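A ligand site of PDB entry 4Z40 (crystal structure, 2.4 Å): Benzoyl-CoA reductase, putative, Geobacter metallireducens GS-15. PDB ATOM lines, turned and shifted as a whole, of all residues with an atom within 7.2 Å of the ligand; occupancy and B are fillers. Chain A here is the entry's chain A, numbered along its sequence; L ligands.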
ATOM      1  N   THR A  73      23.929 -18.436  -0.245  1.00  0.00           N
ATOM      2  CA  THR A  73      22.790 -19.248   0.155  1.00  0.00           C
ATOM      3  C   THR A  73      23.107 -20.206   1.285  1.00  0.00           C
ATOM      4  O   THR A  73      24.065 -20.983   1.198  1.00  0.00           O
ATOM      5  CB  THR A  73      22.265 -20.063  -1.031  1.00  0.00           C
ATOM      6  OG1 THR A  73      21.999 -19.185  -2.131  1.00  0.00           O
ATOM      7  CG2 THR A  73      20.995 -20.800  -0.652  1.00  0.00           C
ATOM      8  N   GLY A  74      22.314 -20.158   2.353  1.00  0.00           N
ATOM      9  CA  GLY A  74      22.451 -21.093   3.455  1.00  0.00           C
ATOM     10  C   GLY A  74      23.708 -20.914   4.304  1.00  0.00           C
ATOM     11  O   GLY A  74      24.084 -21.793   5.080  1.00  0.00           O
ATOM     12  N   CYS A  75      24.359 -19.758   4.179  1.00  0.00           N
ATOM     13  CA  CYS A  75      25.564 -19.503   4.964  1.00  0.00           C
ATOM     14  C   CYS A  75      25.252 -18.739   6.234  1.00  0.00           C
ATOM     15  O   CYS A  75      25.258 -17.509   6.253  1.00  0.00           O
ATOM     16  CB  CYS A  75      26.585 -18.742   4.135  1.00  0.00           C
ATOM     17  SG  CYS A  75      28.232 -18.893   4.782  1.00  0.00           S
ATOM     18  N   ASN A  76      25.008 -19.455   7.325  1.00  0.00           N
ATOM     19  CA  ASN A  76      24.378 -18.832   8.486  1.00  0.00           C
ATOM     20  C   ASN A  76      24.693 -19.482   9.804  1.00  0.00           C
ATOM     21  O   ASN A  76      24.053 -19.190  10.805  1.00  0.00           O
ATOM     22  CB  ASN A  76      22.861 -18.861   8.292  1.00  0.00           C
ATOM     23  CG  ASN A  76      22.377 -20.229   7.853  1.00  0.00           C
ATOM     24  OD1 ASN A  76      22.848 -21.239   8.352  1.00  0.00           O
ATOM     25  ND2 ASN A  76      21.458 -20.254   6.891  1.00  0.00           N
ATOM     26  N   ARG A  77      25.663 -20.390   9.813  1.00  0.00           N
ATOM     27  CA  ARG A  77      25.909 -21.217  10.994  1.00  0.00           C
ATOM     28  C   ARG A  77      26.759 -20.520  12.073  1.00  0.00           C
ATOM     29  O   ARG A  77      27.789 -19.901  11.770  1.00  0.00           O
ATOM     30  CB  ARG A  77      26.584 -22.538  10.598  1.00  0.00           C
ATOM     31  CG  ARG A  77      25.698 -23.762  10.771  1.00  0.00           C
ATOM     32  CD  ARG A  77      24.474 -23.716   9.868  1.00  0.00           C
ATOM     33  NE  ARG A  77      23.475 -24.699  10.279  1.00  0.00           N
ATOM     34  CZ  ARG A  77      22.249 -24.805   9.763  1.00  0.00           C
ATOM     35  NH1 ARG A  77      21.825 -23.988   8.808  1.00  0.00           N
ATOM     36  NH2 ARG A  77      21.429 -25.734  10.226  1.00  0.00           N
ATOM     37  N   GLY A  96      22.253 -23.383  13.419  1.00  0.00           N
ATOM     38  CA  GLY A  96      21.775 -22.666  12.252  1.00  0.00           C
ATOM     39  C   GLY A  96      20.874 -21.503  12.604  1.00  0.00           C
ATOM     40  O   GLY A  96      21.057 -20.852  13.636  1.00  0.00           O
ATOM     41  N   GLY A  97      19.900 -21.234  11.760  1.00  0.00           N
ATOM     42  CA  GLY A  97      18.926 -20.182  12.006  1.00  0.00           C
ATOM     43  C   GLY A  97      19.370 -18.799  11.559  1.00  0.00           C
ATOM     44  O   GLY A  97      19.767 -18.593  10.408  1.00  0.00           O
ATOM     45  N   ARG A 181      14.484 -21.977  15.700  1.00  0.00           N
ATOM     46  CA  ARG A 181      14.508 -23.294  15.037  1.00  0.00           C
ATOM     47  C   ARG A 181      15.918 -23.875  15.002  1.00  0.00           C
ATOM     48  O   ARG A 181      16.223 -24.741  14.177  1.00  0.00           O
ATOM     49  CB  ARG A 181      13.945 -23.190  13.605  1.00  0.00           C
ATOM     50  CG  ARG A 181      14.851 -22.450  12.619  1.00  0.00           C
ATOM     51  CD  ARG A 181      14.874 -23.144  11.267  1.00  0.00           C
ATOM     52  NE  ARG A 181      15.596 -24.420  11.300  1.00  0.00           N
ATOM     53  CZ  ARG A 181      15.791 -25.201  10.244  1.00  0.00           C
ATOM     54  NH1 ARG A 181      15.320 -24.840   9.053  1.00  0.00           N
ATOM     55  NH2 ARG A 181      16.461 -26.330  10.370  1.00  0.00           N
ATOM     56  N   SER A 182      16.773 -23.422  15.911  1.00  0.00           N
ATOM     57  CA  SER A 182      18.159 -23.839  15.876  1.00  0.00           C
ATOM     58  C   SER A 182      18.703 -24.260  17.216  1.00  0.00           C
ATOM     59  O   SER A 182      18.204 -23.845  18.263  1.00  0.00           O
ATOM     60  CB  SER A 182      19.001 -22.704  15.313  1.00  0.00           C
ATOM     61  OG  SER A 182      18.442 -22.311  14.083  1.00  0.00           O
ATOM     62  N   LEU A 246      18.852 -32.291  -1.490  1.00  0.00           N
ATOM     63  CA  LEU A 246      19.660 -31.384  -0.691  1.00  0.00           C
ATOM     64  C   LEU A 246      19.026 -31.115   0.671  1.00  0.00           C
ATOM     65  O   LEU A 246      17.874 -31.470   0.914  1.00  0.00           O
ATOM     66  CB  LEU A 246      19.875 -30.056  -1.435  1.00  0.00           C
ATOM     67  CG  LEU A 246      20.575 -30.142  -2.795  1.00  0.00           C
ATOM     68  CD1 LEU A 246      20.759 -28.762  -3.381  1.00  0.00           C
ATOM     69  CD2 LEU A 246      21.901 -30.865  -2.659  1.00  0.00           C
ATOM     70  N   GLY A 247      19.788 -30.479   1.555  1.00  0.00           N
ATOM     71  CA  GLY A 247      19.316 -30.141   2.892  1.00  0.00           C
ATOM     72  C   GLY A 247      19.775 -31.106   3.966  1.00  0.00           C
ATOM     73  O   GLY A 247      20.439 -32.109   3.678  1.00  0.00           O
ATOM     74  N   SER A 248      19.434 -30.796   5.210  1.00  0.00           N
ATOM     75  CA  SER A 248      19.572 -31.734   6.322  1.00  0.00           C
ATOM     76  C   SER A 248      18.606 -32.881   6.067  1.00  0.00           C
ATOM     77  O   SER A 248      17.720 -32.741   5.223  1.00  0.00           O
ATOM     78  CB  SER A 248      19.274 -31.025   7.647  1.00  0.00           C
ATOM     79  OG  SER A 248      19.976 -29.806   7.745  1.00  0.00           O
ATOM     80  N   GLN A 250      15.667 -34.718   5.533  1.00  0.00           N
ATOM     81  CA  GLN A 250      14.325 -34.165   5.423  1.00  0.00           C
ATOM     82  C   GLN A 250      13.285 -34.990   6.172  1.00  0.00           C
ATOM     83  O   GLN A 250      12.320 -35.464   5.579  1.00  0.00           O
ATOM     84  CB  GLN A 250      13.946 -34.036   3.948  1.00  0.00           C
ATOM     85  CG  GLN A 250      14.875 -33.159   3.126  1.00  0.00           C
ATOM     86  CD  GLN A 250      14.638 -31.679   3.353  1.00  0.00           C
ATOM     87  OE1 GLN A 250      13.673 -31.299   4.008  1.00  0.00           O
ATOM     88  NE2 GLN A 250      15.515 -30.846   2.811  1.00  0.00           N
ATOM     89  N   ILE A 297       9.784 -24.481   7.578  1.00  0.00           N
ATOM     90  CA  ILE A 297      10.448 -23.188   7.587  1.00  0.00           C
ATOM     91  C   ILE A 297      11.960 -23.294   7.403  1.00  0.00           C
ATOM     92  O   ILE A 297      12.553 -24.320   7.721  1.00  0.00           O
ATOM     93  CB  ILE A 297      10.151 -22.418   8.898  1.00  0.00           C
ATOM     94  CG1 ILE A 297      10.694 -23.191  10.102  1.00  0.00           C
ATOM     95  CG2 ILE A 297       8.653 -22.160   9.041  1.00  0.00           C
ATOM     96  CD1 ILE A 297      10.620 -22.421  11.389  1.00  0.00           C
ATOM     97  N   SER A 298      12.564 -22.217   6.903  1.00  0.00           N
ATOM     98  CA  SER A 298      13.987 -22.220   6.563  1.00  0.00           C
ATOM     99  C   SER A 298      14.869 -21.475   7.556  1.00  0.00           C
ATOM    100  O   SER A 298      14.396 -20.614   8.289  1.00  0.00           O
ATOM    101  CB  SER A 298      14.195 -21.574   5.194  1.00  0.00           C
ATOM    102  OG  SER A 298      13.640 -22.344   4.142  1.00  0.00           O
ATOM    103  N   CYS A 299      16.151 -21.824   7.568  1.00  0.00           N
ATOM    104  CA  CYS A 299      17.175 -20.968   8.171  1.00  0.00           C
ATOM    105  C   CYS A 299      17.388 -19.724   7.285  1.00  0.00           C
ATOM    106  O   CYS A 299      16.819 -19.613   6.205  1.00  0.00           O
ATOM    107  CB  CYS A 299      18.482 -21.742   8.325  1.00  0.00           C
ATOM    108  SG  CYS A 299      18.310 -23.253   9.272  1.00  0.00           S
ATOM    109  N   TYR A 300      18.212 -18.787   7.743  1.00  0.00           N
ATOM    110  CA  TYR A 300      18.455 -17.544   7.001  1.00  0.00           C
ATOM    111  C   TYR A 300      18.965 -17.783   5.594  1.00  0.00           C
ATOM    112  O   TYR A 300      19.886 -18.560   5.385  1.00  0.00           O
ATOM    113  CB  TYR A 300      19.440 -16.678   7.761  1.00  0.00           C
ATOM    114  CG  TYR A 300      19.674 -15.287   7.212  1.00  0.00           C
ATOM    115  CD1 TYR A 300      18.657 -14.352   7.197  1.00  0.00           C
ATOM    116  CD2 TYR A 300      20.934 -14.889   6.765  1.00  0.00           C
ATOM    117  CE1 TYR A 300      18.870 -13.066   6.705  1.00  0.00           C
ATOM    118  CE2 TYR A 300      21.168 -13.616   6.286  1.00  0.00           C
ATOM    119  CZ  TYR A 300      20.137 -12.708   6.266  1.00  0.00           C
ATOM    120  OH  TYR A 300      20.353 -11.427   5.792  1.00  0.00           O
ATOM    121  N   ASN A 301      18.327 -17.137   4.620  1.00  0.00           N
ATOM    122  CA  ASN A 301      18.777 -17.149   3.227  1.00  0.00           C
ATOM    123  C   ASN A 301      18.918 -18.559   2.645  1.00  0.00           C
ATOM    124  O   ASN A 301      19.945 -18.892   2.047  1.00  0.00           O
ATOM    125  CB  ASN A 301      20.108 -16.397   3.107  1.00  0.00           C
ATOM    126  CG  ASN A 301      20.467 -16.083   1.656  1.00  0.00           C
ATOM    127  OD1 ASN A 301      19.591 -15.954   0.787  1.00  0.00           O
ATOM    128  ND2 ASN A 301      21.758 -15.970   1.383  1.00  0.00           N
ATOM    129  N   CYS A 302      17.883 -19.382   2.835  1.00  0.00           N
ATOM    130  CA  CYS A 302      17.886 -20.749   2.298  1.00  0.00           C
ATOM    131  C   CYS A 302      16.480 -21.188   1.901  1.00  0.00           C
ATOM    132  O   CYS A 302      15.534 -20.961   2.634  1.00  0.00           O
ATOM    133  CB  CYS A 302      18.466 -21.730   3.307  1.00  0.00           C
ATOM    134  SG  CYS A 302      18.668 -23.416   2.675  1.00  0.00           S
ATOM    135  N   PRO A 303      16.342 -21.819   0.720  1.00  0.00           N
ATOM    136  CA  PRO A 303      15.007 -22.236   0.255  1.00  0.00           C
ATOM    137  C   PRO A 303      14.631 -23.677   0.642  1.00  0.00           C
ATOM    138  O   PRO A 303      13.533 -24.110   0.305  1.00  0.00           O
ATOM    139  CB  PRO A 303      15.137 -22.119  -1.260  1.00  0.00           C
ATOM    140  CG  PRO A 303      16.589 -22.503  -1.508  1.00  0.00           C
ATOM    141  CD  PRO A 303      17.367 -21.976  -0.321  1.00  0.00           C
ATOM    142  N   MET A 304      15.500 -24.392   1.348  1.00  0.00           N
ATOM    143  CA  MET A 304      15.314 -25.822   1.582  1.00  0.00           C
ATOM    144  C   MET A 304      14.290 -26.174   2.671  1.00  0.00           C
ATOM    145  O   MET A 304      13.814 -27.304   2.724  1.00  0.00           O
ATOM    146  CB  MET A 304      16.641 -26.494   1.912  1.00  0.00           C
ATOM    147  CG  MET A 304      17.710 -26.387   0.827  1.00  0.00           C
ATOM    148  SD  MET A 304      17.152 -26.891  -0.810  1.00  0.00           S
ATOM    149  CE  MET A 304      16.553 -28.546  -0.484  1.00  0.00           C
ATOM    150  N   LYS A 305      13.967 -25.201   3.531  1.00  0.00           N
ATOM    151  CA  LYS A 305      13.002 -25.346   4.641  1.00  0.00           C
ATOM    152  C   LYS A 305      12.969 -26.741   5.294  1.00  0.00           C
ATOM    153  O   LYS A 305      11.960 -27.458   5.248  1.00  0.00           O
ATOM    154  CB  LYS A 305      11.585 -24.963   4.164  1.00  0.00           C
ATOM    155  CG  LYS A 305      11.121 -25.601   2.863  1.00  0.00           C
ATOM    156  CD  LYS A 305       9.801 -25.034   2.417  1.00  0.00           C
ATOM    157  CE  LYS A 305       9.311 -25.740   1.173  1.00  0.00           C
ATOM    158  NZ  LYS A 305       7.991 -25.215   0.756  1.00  0.00           N
ATOM    159  N   CYS A 306      14.086 -27.096   5.910  1.00  0.00           N
ATOM    160  CA  CYS A 306      14.244 -28.395   6.552  1.00  0.00           C
ATOM    161  C   CYS A 306      13.471 -28.500   7.855  1.00  0.00           C
ATOM    162  O   CYS A 306      12.979 -29.581   8.199  1.00  0.00           O
ATOM    163  CB  CYS A 306      15.732 -28.666   6.818  1.00  0.00           C
ATOM    164  SG  CYS A 306      16.773 -28.633   5.335  1.00  0.00           S
ATOM    165  N   GLY A 307      13.351 -27.398   8.574  1.00  0.00           N
ATOM    166  CA  GLY A 307      12.697 -27.393   9.870  1.00  0.00           C
ATOM    167  C   GLY A 307      11.180 -27.363   9.779  1.00  0.00           C
ATOM    168  O   GLY A 307      10.613 -27.096   8.723  1.00  0.00           O
ATOM    169  N   LYS A 321      13.703 -30.463  13.712  1.00  0.00           N
ATOM    170  CA  LYS A 321      14.269 -30.913  12.444  1.00  0.00           C
ATOM    171  C   LYS A 321      15.017 -32.219  12.653  1.00  0.00           C
ATOM    172  O   LYS A 321      15.403 -32.556  13.790  1.00  0.00           O
ATOM    173  CB  LYS A 321      15.183 -29.843  11.840  1.00  0.00           C
ATOM    174  CG  LYS A 321      16.667 -29.984  12.157  1.00  0.00           C
ATOM    175  CD  LYS A 321      17.008 -29.687  13.628  1.00  0.00           C
ATOM    176  CE  LYS A 321      16.669 -28.256  14.015  1.00  0.00           C
ATOM    177  NZ  LYS A 321      17.301 -27.895  15.322  1.00  0.00           N
ATOM    178  N   GLN A 533      28.937 -22.178   6.348  1.00  0.00           N
ATOM    179  CA  GLN A 533      28.015 -22.754   5.370  1.00  0.00           C
ATOM    180  C   GLN A 533      27.295 -23.938   5.961  1.00  0.00           C
ATOM    181  O   GLN A 533      27.925 -24.802   6.565  1.00  0.00           O
ATOM    182  CB  GLN A 533      28.769 -23.182   4.121  1.00  0.00           C
ATOM    183  CG  GLN A 533      27.869 -23.710   3.027  1.00  0.00           C
ATOM    184  CD  GLN A 533      26.823 -22.687   2.621  1.00  0.00           C
ATOM    185  OE1 GLN A 533      27.142 -21.563   2.242  1.00  0.00           O
ATOM    186  NE2 GLN A 533      25.555 -23.077   2.723  1.00  0.00           N
ATOM    187  N   CYS A 534      25.984 -24.000   5.779  1.00  0.00           N
ATOM    188  CA  CYS A 534      25.217 -25.153   6.239  1.00  0.00           C
ATOM    189  C   CYS A 534      25.661 -26.401   5.490  1.00  0.00           C
ATOM    190  O   CYS A 534      25.783 -26.390   4.271  1.00  0.00           O
ATOM    191  CB  CYS A 534      23.723 -24.942   6.050  1.00  0.00           C
ATOM    192  SG  CYS A 534      22.729 -26.389   6.564  1.00  0.00           S
ATOM    193  N   ALA A 535      25.865 -27.489   6.219  1.00  0.00           N
ATOM    194  CA  ALA A 535      26.263 -28.736   5.583  1.00  0.00           C
ATOM    195  C   ALA A 535      25.154 -29.299   4.690  1.00  0.00           C
ATOM    196  O   ALA A 535      25.413 -30.146   3.836  1.00  0.00           O
ATOM    197  CB  ALA A 535      26.652 -29.763   6.639  1.00  0.00           C
ATOM    198  N   GLY A 536      23.930 -28.803   4.872  1.00  0.00           N
ATOM    199  CA  GLY A 536      22.793 -29.243   4.073  1.00  0.00           C
ATOM    200  C   GLY A 536      22.922 -28.915   2.600  1.00  0.00           C
ATOM    201  O   GLY A 536      22.229 -29.505   1.761  1.00  0.00           O
ATOM    202  N   LEU A 537      23.804 -27.970   2.281  1.00  0.00           N
ATOM    203  CA  LEU A 537      24.036 -27.556   0.901  1.00  0.00           C
ATOM    204  C   LEU A 537      25.486 -27.824   0.499  1.00  0.00           C
ATOM    205  O   LEU A 537      25.947 -27.394  -0.563  1.00  0.00           O
ATOM    206  CB  LEU A 537      23.716 -26.073   0.730  1.00  0.00           C
ATOM    207  CG  LEU A 537      22.264 -25.654   0.925  1.00  0.00           C
ATOM    208  CD1 LEU A 537      22.124 -24.157   0.720  1.00  0.00           C
ATOM    209  CD2 LEU A 537      21.375 -26.436  -0.036  1.00  0.00           C
HETATM  210 FE1  LIG L   1      18.742 -24.590   7.516  1.00  0.00          FE
HETATM  211 FE2  LIG L   1      18.738 -24.270   4.805  1.00  0.00          FE
HETATM  212 FE3  LIG L   1      17.889 -26.610   5.767  1.00  0.00          FE
HETATM  213 FE4  LIG L   1      20.522 -25.973   5.926  1.00  0.00          FE
HETATM  214  S1  LIG L   1      19.325 -26.357   3.992  1.00  0.00           S
HETATM  215  S2  LIG L   1      19.228 -26.820   7.627  1.00  0.00           S
HETATM  216  S3  LIG L   1      20.432 -23.693   6.253  1.00  0.00           S
HETATM  217  S4  LIG L   1      16.887 -24.565   6.146  1.00  0.00           S
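Merely in contact with the ligand: Met 304, Ser 298, Gly 247 and Lys 305.
Hydrophobic or aromatic side chains within 4 Å of the ligand: Met 304.
N of Cys 299 lies close to S4 of the ligand, at 3.2 Å.
The side-chain sulfur (SG) of Cys 299 is bound to an iron atom (FE1) of the ligand (2.2 Å).
The side-chain sulfur of Cys 302 is bound to an iron atom (FE2) of the ligand, at 2.3 Å.
SG of Cys 534 binds FE4 of the ligand, at 2.3 Å.
N of Cys 306 sits close to S4 of the ligand (3.8 Å).
An iron atom (FE3) of the ligand is bound by the side-chain sulfur (SG) of Cys 306, at 2.4 Å.
The guanidinium group (NH1) of Arg 77 lies close to a sulfur (S3) of the ligand (2.9 Å).
A sulfur (S2) of the ligand sits close to the side-chain hydroxyl of Ser 248 (3.1 Å).
S4 of the ligand lies close to NH1 of Arg 181 (3.3 Å).
The side-chain amide nitrogen (ND2) of Asn 76 lies close to a sulfur (S3) of the ligand, at 3.6 Å.
The guanidinium group (NH1) of Arg 77 sits close to the side-chain sulfur (SG) of Cys 299 (3.6 Å).
SG of Cys 299 sits close to NH1 of Arg 181 (3.4 Å).
SG of Cys 302 sits close to N of Met 304.
The guanidinium group (NH1) of Arg 77 lies close to the side-chain sulfur (SG) of Cys 534, 3.4 Å away.
The backbone NH (N) of Cys 534 sits at hydrogen-bond distance from the backbone carbonyl oxygen (O) of Gly 74 (3.0 Å).
The side-chain amide nitrogen (NE2) of Gln 250 sits close to the side-chain sulfur (SG) of Cys 306 (3.6 Å).
OD1 of Asn 76 sits at hydrogen-bond distance from NH1 of Arg 77 (3.0 Å).
The backbone carbonyl oxygen (O) of Gly 536 sits at hydrogen-bond distance from the backbone NH (N) of Gly 247.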
